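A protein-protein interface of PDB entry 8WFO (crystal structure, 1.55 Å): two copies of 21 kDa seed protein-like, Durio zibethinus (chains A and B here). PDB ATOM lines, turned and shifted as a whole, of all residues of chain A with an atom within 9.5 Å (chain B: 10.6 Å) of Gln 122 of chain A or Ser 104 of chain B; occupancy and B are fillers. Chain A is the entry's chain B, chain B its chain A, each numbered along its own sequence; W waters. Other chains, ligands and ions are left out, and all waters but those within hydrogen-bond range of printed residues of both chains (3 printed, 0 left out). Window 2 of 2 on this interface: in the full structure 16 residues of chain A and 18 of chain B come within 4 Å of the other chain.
Ser 120 of chain A touches none of the printed residues of chain B.
Pro 121 of chain A touches three residues of chain B.
Gln 122 of chain A touches two residues of chain B.
No residue of chain B comes within 4 Å of Thr 123 of chain A.
Printed residues of chain B within 4 Å of Leu 124 of chain A: Tyr 101.
Of the printed residues of chain B, Gln 125 of chain A touches Tyr 101 (3.8 Å) and Thr 103 (3.4 Å).
Of the printed residues of chain A, Tyr 101 of chain B touches Pro 121 (2.7 Å), Leu 124 (3.4 Å) and Gln 125 (3.8 Å).
Of chain A, only Gln 122 comes within 4 Å of Ser 104 of chain B.
Thr 105 of chain B touches none of the printed residues of chain A.
Of the printed residues of chain A, Gly 106 of chain B touches Pro 121.
The side-chain hydroxyl (OH) of Tyr 101 of chain B is in hydrogen-bond range of the backbone carbonyl oxygen (O) of Pro 121 of chain A (2.7 Å).
NE2 of Gln 122 of chain A sits at hydrogen-bond distance from O of Thr 103 of chain B, 2.8 Å away.
O of Ser 104 of chain B is in hydrogen-bond range of NE2 of Gln 122 of chain A (3.4 Å).
The side-chain amide oxygen (OE1) of Gln 125 of chain A lies within hydrogen-bond range of the side-chain amino group (NZ) of Lys 97 of chain A.
SG of Cys 147 of chain A is disulfide-bonded to SG of Cys 150 of chain A, at 2.1 Å.
OG of Ser 120 of chain A lies close to N of Gln 122 of chain A (3.3 Å).
N of Ile 98 of chain A lies within hydrogen-bond range of O of Gln 125 of chain A (3.0 Å).
Among the printed residues, pairs that only touch across the chains: Pro 121 of chain A with Thr 103 of chain B (3.95 Å), Pro 121 of chain A with Gly 106 of chain B (3.7 Å), Leu 124 of chain A with Tyr 101 of chain B (3.4 Å), Gln 125 of chain A with Tyr 101 of chain B (3.8 Å) and Gln 125 of chain A with Thr 103 of chain B (3.4 Å).
Hydrophobic or aromatic side chains of chain B within 4 Å of the printed part of chain A: Tyr 101.
No position is printed for both chains.
Of the 8 pairs that touch across the chains among the printed residues, none has its exchanged pair printed and touching as well.
Water W3 bridges the backbone carbonyl oxygen (O) of Tyr 101 of chain B (2.9 Å) and the side-chain amide nitrogen (NE2) of Gln 125 of chain A (3.0 Å).
Water W2 lies within hydrogen-bond range of the side-chain amide nitrogen of Gln 122 of chain A and the backbone carbonyl oxygen of Ser 104 of chain B.
Water W1 lies within hydrogen-bond range of NZ of Lys 107 of chain B (3.4 Å), O of Gly 106 of chain B (3.4 Å) and SG of Cys 150 of chain A (3.8 Å).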
ATOM      1  N   LYS A  97      12.940  20.551 -37.837  1.00  0.00           N
ATOM      2  CA  LYS A  97      13.540  20.853 -36.545  1.00  0.00           C
ATOM      3  C   LYS A  97      12.778  22.005 -35.918  1.00  0.00           C
ATOM      4  O   LYS A  97      12.129  22.794 -36.602  1.00  0.00           O
ATOM      5  CB  LYS A  97      15.029  21.202 -36.665  1.00  0.00           C
ATOM      6  CG  LYS A  97      15.281  22.545 -37.336  1.00  0.00           C
ATOM      7  CD  LYS A  97      16.712  23.075 -37.162  1.00  0.00           C
ATOM      8  CE  LYS A  97      17.307  22.767 -35.816  1.00  0.00           C
ATOM      9  NZ  LYS A  97      18.533  23.578 -35.624  1.00  0.00           N
ATOM     10  N   ILE A  98      12.883  22.099 -34.601  1.00  0.00           N
ATOM     11  CA  ILE A  98      12.293  23.216 -33.874  1.00  0.00           C
ATOM     12  C   ILE A  98      13.247  24.397 -33.966  1.00  0.00           C
ATOM     13  O   ILE A  98      14.454  24.259 -33.731  1.00  0.00           O
ATOM     14  CB  ILE A  98      11.993  22.847 -32.414  1.00  0.00           C
ATOM     15  CG1 ILE A  98      10.945  21.752 -32.373  1.00  0.00           C
ATOM     16  CG2 ILE A  98      11.493  24.075 -31.650  1.00  0.00           C
ATOM     17  CD1 ILE A  98       9.673  22.135 -33.108  1.00  0.00           C
ATOM     18  N   ASP A 113      16.217  22.385 -42.072  1.00  0.00           N
ATOM     19  CA  ASP A 113      17.657  22.323 -41.811  1.00  0.00           C
ATOM     20  C   ASP A 113      17.969  21.522 -40.542  1.00  0.00           C
ATOM     21  O   ASP A 113      18.975  21.752 -39.860  1.00  0.00           O
ATOM     22  CB  ASP A 113      18.308  23.715 -41.735  1.00  0.00           C
ATOM     23  CG  ASP A 113      19.791  23.674 -42.109  1.00  0.00           C
ATOM     24  OD1 ASP A 113      20.199  22.748 -42.858  1.00  0.00           O
ATOM     25  OD2 ASP A 113      20.564  24.551 -41.648  1.00  0.00           O
ATOM     26  N   GLY A 114      17.123  20.539 -40.230  1.00  0.00           N
ATOM     27  CA  GLY A 114      17.435  19.582 -39.200  1.00  0.00           C
ATOM     28  C   GLY A 114      18.454  18.550 -39.666  1.00  0.00           C
ATOM     29  O   GLY A 114      18.986  18.590 -40.780  1.00  0.00           O
ATOM     30  N   VAL A 115      18.721  17.597 -38.776  1.00  0.00           N
ATOM     31  CA  VAL A 115      19.753  16.588 -38.982  1.00  0.00           C
ATOM     32  C   VAL A 115      19.141  15.216 -38.744  1.00  0.00           C
ATOM     33  O   VAL A 115      18.272  15.060 -37.881  1.00  0.00           O
ATOM     34  CB  VAL A 115      20.954  16.837 -38.040  1.00  0.00           C
ATOM     35  CG1 VAL A 115      21.966  15.716 -38.128  1.00  0.00           C
ATOM     36  CG2 VAL A 115      21.612  18.167 -38.390  1.00  0.00           C
ATOM     37  N   ILE A 116      19.574  14.225 -39.531  1.00  0.00           N
ATOM     38  CA  ILE A 116      19.130  12.843 -39.352  1.00  0.00           C
ATOM     39  C   ILE A 116      20.128  12.100 -38.475  1.00  0.00           C
ATOM     40  O   ILE A 116      21.343  12.175 -38.698  1.00  0.00           O
ATOM     41  CB  ILE A 116      18.962  12.140 -40.709  1.00  0.00           C
ATOM     42  CG1 ILE A 116      17.799  12.769 -41.476  1.00  0.00           C
ATOM     43  CG2 ILE A 116      18.749  10.649 -40.507  1.00  0.00           C
ATOM     44  CD1 ILE A 116      17.535  12.151 -42.833  1.00  0.00           C
ATOM     45  N   GLY A 117      19.616  11.377 -37.482  1.00  0.00           N
ATOM     46  CA  GLY A 117      20.442  10.476 -36.701  1.00  0.00           C
ATOM     47  C   GLY A 117      21.293  11.203 -35.675  1.00  0.00           C
ATOM     48  O   GLY A 117      21.055  12.368 -35.331  1.00  0.00           O
ATOM     49  N   ASN A 118      22.303  10.489 -35.181  1.00  0.00           N
ATOM     50  CA  ASN A 118      23.185  10.975 -34.126  1.00  0.00           C
ATOM     51  C   ASN A 118      22.391  11.543 -32.944  1.00  0.00           C
ATOM     52  O   ASN A 118      22.525  12.725 -32.614  1.00  0.00           O
ATOM     53  CB  ASN A 118      24.158  12.016 -34.667  1.00  0.00           C
ATOM     54  CG  ASN A 118      25.180  12.473 -33.624  1.00  0.00           C
ATOM     55  OD1 ASN A 118      25.439  11.779 -32.634  1.00  0.00           O
ATOM     56  ND2 ASN A 118      25.702  13.677 -33.804  1.00  0.00           N
ATOM     57  N   PRO A 119      21.562  10.728 -32.289  1.00  0.00           N
ATOM     58  CA  PRO A 119      20.830  11.222 -31.109  1.00  0.00           C
ATOM     59  C   PRO A 119      21.810  11.730 -30.065  1.00  0.00           C
ATOM     60  O   PRO A 119      22.701  11.003 -29.617  1.00  0.00           O
ATOM     61  CB  PRO A 119      20.063   9.991 -30.619  1.00  0.00           C
ATOM     62  CG  PRO A 119      20.786   8.816 -31.227  1.00  0.00           C
ATOM     63  CD  PRO A 119      21.327   9.293 -32.529  1.00  0.00           C
ATOM     64  N   SER A 120      21.649  12.994 -29.688  1.00  0.00           N
ATOM     65  CA  SER A 120      22.657  13.667 -28.886  1.00  0.00           C
ATOM     66  C   SER A 120      22.162  15.062 -28.555  1.00  0.00           C
ATOM     67  O   SER A 120      21.186  15.527 -29.159  1.00  0.00           O
ATOM     68  CB  SER A 120      23.975  13.754 -29.654  1.00  0.00           C
ATOM     69  OG  SER A 120      23.827  14.588 -30.792  1.00  0.00           O
ATOM     70  N   PRO A 121      22.811  15.776 -27.635  1.00  0.00           N
ATOM     71  CA  PRO A 121      22.468  17.192 -27.459  1.00  0.00           C
ATOM     72  C   PRO A 121      22.556  17.988 -28.743  1.00  0.00           C
ATOM     73  O   PRO A 121      21.752  18.907 -28.949  1.00  0.00           O
ATOM     74  CB  PRO A 121      23.485  17.674 -26.408  1.00  0.00           C
ATOM     75  CG  PRO A 121      23.952  16.445 -25.727  1.00  0.00           C
ATOM     76  CD  PRO A 121      23.889  15.345 -26.728  1.00  0.00           C
ATOM     77  N   GLN A 122      23.491  17.648 -29.636  1.00  0.00           N
ATOM     78  CA  GLN A 122      23.683  18.449 -30.836  1.00  0.00           C
ATOM     79  C   GLN A 122      22.473  18.379 -31.757  1.00  0.00           C
ATOM     80  O   GLN A 122      22.177  19.353 -32.456  1.00  0.00           O
ATOM     81  CB  GLN A 122      24.944  18.005 -31.585  1.00  0.00           C
ATOM     82  CG  GLN A 122      26.265  18.390 -30.902  1.00  0.00           C
ATOM     83  CD  GLN A 122      26.435  17.736 -29.547  1.00  0.00           C
ATOM     84  OE1 GLN A 122      26.416  16.510 -29.441  1.00  0.00           O
ATOM     85  NE2 GLN A 122      26.632  18.552 -28.497  1.00  0.00           N
ATOM     86  N   THR A 123      21.756  17.256 -31.767  1.00  0.00           N
ATOM     87  CA  THR A 123      20.644  17.075 -32.696  1.00  0.00           C
ATOM     88  C   THR A 123      19.284  17.159 -32.012  1.00  0.00           C
ATOM     89  O   THR A 123      18.280  16.793 -32.626  1.00  0.00           O
ATOM     90  CB  THR A 123      20.749  15.730 -33.425  1.00  0.00           C
ATOM     91  OG1 THR A 123      20.645  14.649 -32.482  1.00  0.00           O
ATOM     92  CG2 THR A 123      22.059  15.628 -34.222  1.00  0.00           C
ATOM     93  N   LEU A 124      19.233  17.634 -30.762  1.00  0.00           N
ATOM     94  CA  LEU A 124      18.015  17.567 -29.953  1.00  0.00           C
ATOM     95  C   LEU A 124      16.805  18.181 -30.654  1.00  0.00           C
ATOM     96  O   LEU A 124      15.679  17.678 -30.525  1.00  0.00           O
ATOM     97  CB  LEU A 124      18.256  18.258 -28.610  1.00  0.00           C
ATOM     98  CG  LEU A 124      17.301  17.919 -27.470  1.00  0.00           C
ATOM     99  CD1 LEU A 124      17.295  16.442 -27.197  1.00  0.00           C
ATOM    100  CD2 LEU A 124      17.745  18.674 -26.232  1.00  0.00           C
ATOM    101  N   GLN A 125      17.014  19.264 -31.400  1.00  0.00           N
ATOM    102  CA  GLN A 125      15.901  19.963 -32.029  1.00  0.00           C
ATOM    103  C   GLN A 125      15.304  19.207 -33.212  1.00  0.00           C
ATOM    104  O   GLN A 125      14.267  19.640 -33.723  1.00  0.00           O
ATOM    105  CB  GLN A 125      16.354  21.348 -32.500  1.00  0.00           C
ATOM    106  CG  GLN A 125      16.828  22.252 -31.379  1.00  0.00           C
ATOM    107  CD  GLN A 125      17.793  23.311 -31.842  1.00  0.00           C
ATOM    108  OE1 GLN A 125      18.838  23.008 -32.421  1.00  0.00           O
ATOM    109  NE2 GLN A 125      17.472  24.581 -31.538  1.00  0.00           N
ATOM    110  N   SER A 126      15.911  18.101 -33.653  1.00  0.00           N
ATOM    111  CA  SER A 126      15.429  17.354 -34.815  1.00  0.00           C
ATOM    112  C   SER A 126      14.605  16.110 -34.461  1.00  0.00           C
ATOM    113  O   SER A 126      14.233  15.360 -35.373  1.00  0.00           O
ATOM    114  CB  SER A 126      16.615  16.939 -35.700  1.00  0.00           C
ATOM    115  OG  SER A 126      17.214  18.059 -36.339  1.00  0.00           O
ATOM    116  N   TRP A 127      14.294  15.869 -33.186  1.00  0.00           N
ATOM    117  CA  TRP A 127      13.618  14.637 -32.768  1.00  0.00           C
ATOM    118  C   TRP A 127      12.164  14.924 -32.408  1.00  0.00           C
ATOM    119  O   TRP A 127      11.889  15.760 -31.535  1.00  0.00           O
ATOM    120  CB  TRP A 127      14.342  13.991 -31.585  1.00  0.00           C
ATOM    121  CG  TRP A 127      15.709  13.522 -31.967  1.00  0.00           C
ATOM    122  CD1 TRP A 127      16.889  14.172 -31.737  1.00  0.00           C
ATOM    123  CD2 TRP A 127      16.041  12.324 -32.680  1.00  0.00           C
ATOM    124  NE1 TRP A 127      17.940  13.455 -32.259  1.00  0.00           N
ATOM    125  CE2 TRP A 127      17.446  12.315 -32.846  1.00  0.00           C
ATOM    126  CE3 TRP A 127      15.288  11.262 -33.205  1.00  0.00           C
ATOM    127  CZ2 TRP A 127      18.118  11.284 -33.507  1.00  0.00           C
ATOM    128  CZ3 TRP A 127      15.960  10.234 -33.870  1.00  0.00           C
ATOM    129  CH2 TRP A 127      17.356  10.251 -34.012  1.00  0.00           C
ATOM    130  N   VAL A 146      16.138  11.742 -26.106  1.00  0.00           N
ATOM    131  CA  VAL A 146      17.440  11.196 -26.485  1.00  0.00           C
ATOM    132  C   VAL A 146      18.583  11.684 -25.609  1.00  0.00           C
ATOM    133  O   VAL A 146      19.686  11.134 -25.702  1.00  0.00           O
ATOM    134  CB  VAL A 146      17.786  11.530 -27.950  1.00  0.00           C
ATOM    135  CG1 VAL A 146      16.730  10.959 -28.889  1.00  0.00           C
ATOM    136  CG2 VAL A 146      17.929  13.026 -28.148  1.00  0.00           C
ATOM    137  N   CYS A 147      18.365  12.711 -24.782  1.00  0.00           N
ATOM    138  CA  CYS A 147      19.397  13.275 -23.905  1.00  0.00           C
ATOM    139  C   CYS A 147      18.765  13.462 -22.529  1.00  0.00           C
ATOM    140  O   CYS A 147      18.077  14.460 -22.298  1.00  0.00           O
ATOM    141  CB  CYS A 147      19.936  14.603 -24.454  1.00  0.00           C
ATOM    142  SG  CYS A 147      21.053  15.514 -23.292  1.00  0.00           S
ATOM    143  N   CYS A 150      19.437  16.789 -20.658  1.00  0.00           N
ATOM    144  CA  CYS A 150      19.157  18.033 -21.358  1.00  0.00           C
ATOM    145  C   CYS A 150      17.790  18.536 -20.941  1.00  0.00           C
ATOM    146  O   CYS A 150      16.818  17.773 -20.923  1.00  0.00           O
ATOM    147  CB  CYS A 150      19.192  17.859 -22.879  1.00  0.00           C
ATOM    148  SG  CYS A 150      20.822  17.545 -23.589  1.00  0.00           S
ATOM    149  N   LEU B  38      32.923  35.496 -23.195  1.00  0.00           N
ATOM    150  CA  LEU B  38      33.492  34.320 -23.828  1.00  0.00           C
ATOM    151  C   LEU B  38      34.720  34.706 -24.651  1.00  0.00           C
ATOM    152  O   LEU B  38      34.998  35.882 -24.890  1.00  0.00           O
ATOM    153  CB  LEU B  38      32.454  33.650 -24.715  1.00  0.00           C
ATOM    154  CG  LEU B  38      31.235  33.124 -23.967  1.00  0.00           C
ATOM    155  CD1 LEU B  38      30.092  32.916 -24.943  1.00  0.00           C
ATOM    156  CD2 LEU B  38      31.584  31.854 -23.222  1.00  0.00           C
ATOM    157  N   ASP B  40      35.292  33.874 -27.959  1.00  0.00           N
ATOM    158  CA  ASP B  40      34.887  34.356 -29.274  1.00  0.00           C
ATOM    159  C   ASP B  40      33.849  35.461 -29.199  1.00  0.00           C
ATOM    160  O   ASP B  40      33.481  36.018 -30.240  1.00  0.00           O
ATOM    161  CB  ASP B  40      34.327  33.216 -30.140  1.00  0.00           C
ATOM    162  CG  ASP B  40      33.157  32.484 -29.490  1.00  0.00           C
ATOM    163  OD1 ASP B  40      32.818  32.772 -28.323  1.00  0.00           O
ATOM    164  OD2 ASP B  40      32.554  31.623 -30.168  1.00  0.00           O
ATOM    165  N   ASP B  99      19.269  32.318 -23.253  1.00  0.00           N
ATOM    166  CA  ASP B  99      19.816  32.269 -24.603  1.00  0.00           C
ATOM    167  C   ASP B  99      19.036  31.272 -25.468  1.00  0.00           C
ATOM    168  O   ASP B  99      18.185  30.510 -24.992  1.00  0.00           O
ATOM    169  CB  ASP B  99      21.293  31.879 -24.531  1.00  0.00           C
ATOM    170  CG  ASP B  99      22.105  32.339 -25.734  1.00  0.00           C
ATOM    171  OD1 ASP B  99      21.554  32.957 -26.680  1.00  0.00           O
ATOM    172  OD2 ASP B  99      23.327  32.076 -25.723  1.00  0.00           O
ATOM    173  N   ASP B 100      19.342  31.296 -26.761  1.00  0.00           N
ATOM    174  CA  ASP B 100      18.912  30.232 -27.663  1.00  0.00           C
ATOM    175  C   ASP B 100      19.653  28.952 -27.302  1.00  0.00           C
ATOM    176  O   ASP B 100      20.769  28.984 -26.786  1.00  0.00           O
ATOM    177  CB  ASP B 100      19.214  30.619 -29.114  1.00  0.00           C
ATOM    178  CG  ASP B 100      18.377  31.777 -29.598  1.00  0.00           C
ATOM    179  OD1 ASP B 100      17.194  31.891 -29.233  1.00  0.00           O
ATOM    180  OD2 ASP B 100      18.959  32.661 -30.258  1.00  0.00           O
ATOM    181  N   TYR B 101      19.024  27.813 -27.582  1.00  0.00           N
ATOM    182  CA  TYR B 101      19.634  26.523 -27.277  1.00  0.00           C
ATOM    183  C   TYR B 101      21.022  26.407 -27.897  1.00  0.00           C
ATOM    184  O   TYR B 101      21.224  26.736 -29.070  1.00  0.00           O
ATOM    185  CB  TYR B 101      18.739  25.404 -27.807  1.00  0.00           C
ATOM    186  CG  TYR B 101      19.268  24.014 -27.534  1.00  0.00           C
ATOM    187  CD1 TYR B 101      19.326  23.508 -26.228  1.00  0.00           C
ATOM    188  CD2 TYR B 101      19.699  23.203 -28.581  1.00  0.00           C
ATOM    189  CE1 TYR B 101      19.808  22.240 -25.979  1.00  0.00           C
ATOM    190  CE2 TYR B 101      20.183  21.937 -28.337  1.00  0.00           C
ATOM    191  CZ  TYR B 101      20.231  21.458 -27.047  1.00  0.00           C
ATOM    192  OH  TYR B 101      20.705  20.191 -26.816  1.00  0.00           O
ATOM    193  N   ASP B 102      21.981  25.938 -27.098  1.00  0.00           N
ATOM    194  CA  ASP B 102      23.377  25.800 -27.513  1.00  0.00           C
ATOM    195  C   ASP B 102      23.606  24.346 -27.905  1.00  0.00           C
ATOM    196  O   ASP B 102      23.760  23.479 -27.041  1.00  0.00           O
ATOM    197  CB  ASP B 102      24.303  26.223 -26.377  1.00  0.00           C
ATOM    198  CG  ASP B 102      25.772  26.083 -26.734  1.00  0.00           C
ATOM    199  OD1 ASP B 102      26.096  25.809 -27.906  1.00  0.00           O
ATOM    200  OD2 ASP B 102      26.615  26.242 -25.823  1.00  0.00           O
ATOM    201  N   THR B 103      23.593  24.068 -29.216  1.00  0.00           N
ATOM    202  CA  THR B 103      23.747  22.681 -29.642  1.00  0.00           C
ATOM    203  C   THR B 103      25.096  22.105 -29.239  1.00  0.00           C
ATOM    204  O   THR B 103      25.218  20.889 -29.068  1.00  0.00           O
ATOM    205  CB  THR B 103      23.553  22.540 -31.158  1.00  0.00           C
ATOM    206  OG1 THR B 103      24.524  23.327 -31.857  1.00  0.00           O
ATOM    207  CG2 THR B 103      22.159  22.992 -31.545  1.00  0.00           C
ATOM    208  N   SER B 104      26.116  22.945 -29.073  1.00  0.00           N
ATOM    209  CA  SER B 104      27.437  22.394 -28.798  1.00  0.00           C
ATOM    210  C   SER B 104      27.565  21.871 -27.375  1.00  0.00           C
ATOM    211  O   SER B 104      28.462  21.066 -27.108  1.00  0.00           O
ATOM    212  CB  SER B 104      28.521  23.439 -29.079  1.00  0.00           C
ATOM    213  OG  SER B 104      28.468  24.528 -28.166  1.00  0.00           O
ATOM    214  N   THR B 105      26.693  22.298 -26.455  1.00  0.00           N
ATOM    215  CA  THR B 105      26.751  21.856 -25.068  1.00  0.00           C
ATOM    216  C   THR B 105      25.466  21.224 -24.568  1.00  0.00           C
ATOM    217  O   THR B 105      25.490  20.573 -23.516  1.00  0.00           O
ATOM    218  CB  THR B 105      27.072  23.036 -24.134  1.00  0.00           C
ATOM    219  OG1 THR B 105      26.013  24.002 -24.235  1.00  0.00           O
ATOM    220  CG2 THR B 105      28.390  23.687 -24.511  1.00  0.00           C
ATOM    221  N   GLY B 106      24.350  21.411 -25.264  1.00  0.00           N
ATOM    222  CA  GLY B 106      23.079  20.977 -24.738  1.00  0.00           C
ATOM    223  C   GLY B 106      22.493  21.873 -23.677  1.00  0.00           C
ATOM    224  O   GLY B 106      21.594  21.445 -22.952  1.00  0.00           O
ATOM    225  N   LYS B 107      22.959  23.114 -23.573  1.00  0.00           N
ATOM    226  CA  LYS B 107      22.541  24.001 -22.498  1.00  0.00           C
ATOM    227  C   LYS B 107      21.731  25.179 -23.014  1.00  0.00           C
ATOM    228  O   LYS B 107      21.937  25.661 -24.138  1.00  0.00           O
ATOM    229  CB  LYS B 107      23.754  24.538 -21.744  1.00  0.00           C
ATOM    230  CG  LYS B 107      24.559  23.462 -21.061  1.00  0.00           C
ATOM    231  CD  LYS B 107      23.805  22.912 -19.893  1.00  0.00           C
ATOM    232  CE  LYS B 107      24.697  22.006 -19.065  1.00  0.00           C
ATOM    233  NZ  LYS B 107      23.922  20.941 -18.375  1.00  0.00           N
ATOM    234  N   TRP B 108      20.815  25.630 -22.161  1.00  0.00           N
ATOM    235  CA  TRP B 108      20.131  26.912 -22.267  1.00  0.00           C
ATOM    236  C   TRP B 108      20.802  27.852 -21.266  1.00  0.00           C
ATOM    237  O   TRP B 108      20.466  27.849 -20.073  1.00  0.00           O
ATOM    238  CB  TRP B 108      18.648  26.763 -21.943  1.00  0.00           C
ATOM    239  CG  TRP B 108      17.864  25.810 -22.796  1.00  0.00           C
ATOM    240  CD1 TRP B 108      17.678  24.481 -22.576  1.00  0.00           C
ATOM    241  CD2 TRP B 108      17.129  26.133 -23.975  1.00  0.00           C
ATOM    242  NE1 TRP B 108      16.863  23.941 -23.559  1.00  0.00           N
ATOM    243  CE2 TRP B 108      16.513  24.944 -24.424  1.00  0.00           C
ATOM    244  CE3 TRP B 108      16.923  27.314 -24.692  1.00  0.00           C
ATOM    245  CZ2 TRP B 108      15.709  24.907 -25.558  1.00  0.00           C
ATOM    246  CZ3 TRP B 108      16.131  27.273 -25.824  1.00  0.00           C
ATOM    247  CH2 TRP B 108      15.522  26.078 -26.237  1.00  0.00           C
ATOM    248  N   TRP B 109      21.754  28.644 -21.751  1.00  0.00           N
ATOM    249  CA  TRP B 109      22.550  29.498 -20.870  1.00  0.00           C
ATOM    250  C   TRP B 109      21.769  30.729 -20.428  1.00  0.00           C
ATOM    251  O   TRP B 109      20.911  31.241 -21.149  1.00  0.00           O
ATOM    252  CB  TRP B 109      23.827  29.960 -21.581  1.00  0.00           C
ATOM    253  CG  TRP B 109      24.749  28.873 -22.001  1.00  0.00           C
ATOM    254  CD1 TRP B 109      25.048  28.506 -23.296  1.00  0.00           C
ATOM    255  CD2 TRP B 109      25.507  28.005 -21.153  1.00  0.00           C
ATOM    256  NE1 TRP B 109      25.939  27.462 -23.287  1.00  0.00           N
ATOM    257  CE2 TRP B 109      26.244  27.138 -21.990  1.00  0.00           C
ATOM    258  CE3 TRP B 109      25.653  27.887 -19.763  1.00  0.00           C
ATOM    259  CZ2 TRP B 109      27.095  26.153 -21.480  1.00  0.00           C
ATOM    260  CZ3 TRP B 109      26.489  26.901 -19.265  1.00  0.00           C
ATOM    261  CH2 TRP B 109      27.212  26.062 -20.119  1.00  0.00           C
ATOM    262  N   GLY B 161      30.203  24.406 -15.375  1.00  0.00           N
ATOM    263  CA  GLY B 161      31.479  24.865 -15.879  1.00  0.00           C
ATOM    264  C   GLY B 161      31.556  24.667 -17.382  1.00  0.00           C
ATOM    265  O   GLY B 161      31.125  23.647 -17.918  1.00  0.00           O
ATOM    266  N   HIS B 162      32.089  25.673 -18.068  1.00  0.00           N
ATOM    267  CA  HIS B 162      32.295  25.541 -19.502  1.00  0.00           C
ATOM    268  C   HIS B 162      33.408  26.479 -19.929  1.00  0.00           C
ATOM    269  O   HIS B 162      33.368  27.672 -19.613  1.00  0.00           O
ATOM    270  CB  HIS B 162      31.024  25.852 -20.299  1.00  0.00           C
ATOM    271  CG  HIS B 162      31.143  25.502 -21.750  1.00  0.00           C
ATOM    272  ND1 HIS B 162      30.879  26.401 -22.760  1.00  0.00           N
ATOM    273  CD2 HIS B 162      31.521  24.351 -22.357  1.00  0.00           C
ATOM    274  CE1 HIS B 162      31.087  25.818 -23.928  1.00  0.00           C
ATOM    275  NE2 HIS B 162      31.476  24.573 -23.711  1.00  0.00           N
ATOM    276  N   ASP B 163      34.388  25.934 -20.654  1.00  0.00           N
ATOM    277  CA  ASP B 163      35.487  26.711 -21.226  1.00  0.00           C
ATOM    278  C   ASP B 163      36.164  27.581 -20.168  1.00  0.00           C
ATOM    279  O   ASP B 163      36.440  28.763 -20.376  1.00  0.00           O
ATOM    280  CB  ASP B 163      35.001  27.545 -22.411  1.00  0.00           C
ATOM    281  CG  ASP B 163      34.570  26.678 -23.598  1.00  0.00           C
ATOM    282  OD1 ASP B 163      34.860  25.462 -23.588  1.00  0.00           O
ATOM    283  OD2 ASP B 163      33.945  27.213 -24.537  1.00  0.00           O
ATOM    284  N   ARG B 167      29.310  29.114 -15.474  1.00  0.00           N
ATOM    285  CA  ARG B 167      28.140  29.780 -16.031  1.00  0.00           C
ATOM    286  C   ARG B 167      26.866  29.295 -15.339  1.00  0.00           C
ATOM    287  O   ARG B 167      26.872  28.334 -14.570  1.00  0.00           O
ATOM    288  CB  ARG B 167      28.042  29.518 -17.540  1.00  0.00           C
ATOM    289  CG  ARG B 167      29.207  30.075 -18.336  1.00  0.00           C
ATOM    290  CD  ARG B 167      28.882  30.060 -19.839  1.00  0.00           C
ATOM    291  NE  ARG B 167      27.747  30.928 -20.122  1.00  0.00           N
ATOM    292  CZ  ARG B 167      27.299  31.199 -21.339  1.00  0.00           C
ATOM    293  NH1 ARG B 167      27.833  30.634 -22.409  1.00  0.00           N
ATOM    294  NH2 ARG B 167      26.314  32.081 -21.483  1.00  0.00           N
HETATM  295  O   HOH W   1      23.173  19.063 -21.084  1.00  0.00           O
HETATM  296  O   HOH W   2      27.730  18.130 -25.418  1.00  0.00           O
HETATM  297  O   HOH W   3      19.643  26.695 -31.475  1.00  0.00           O
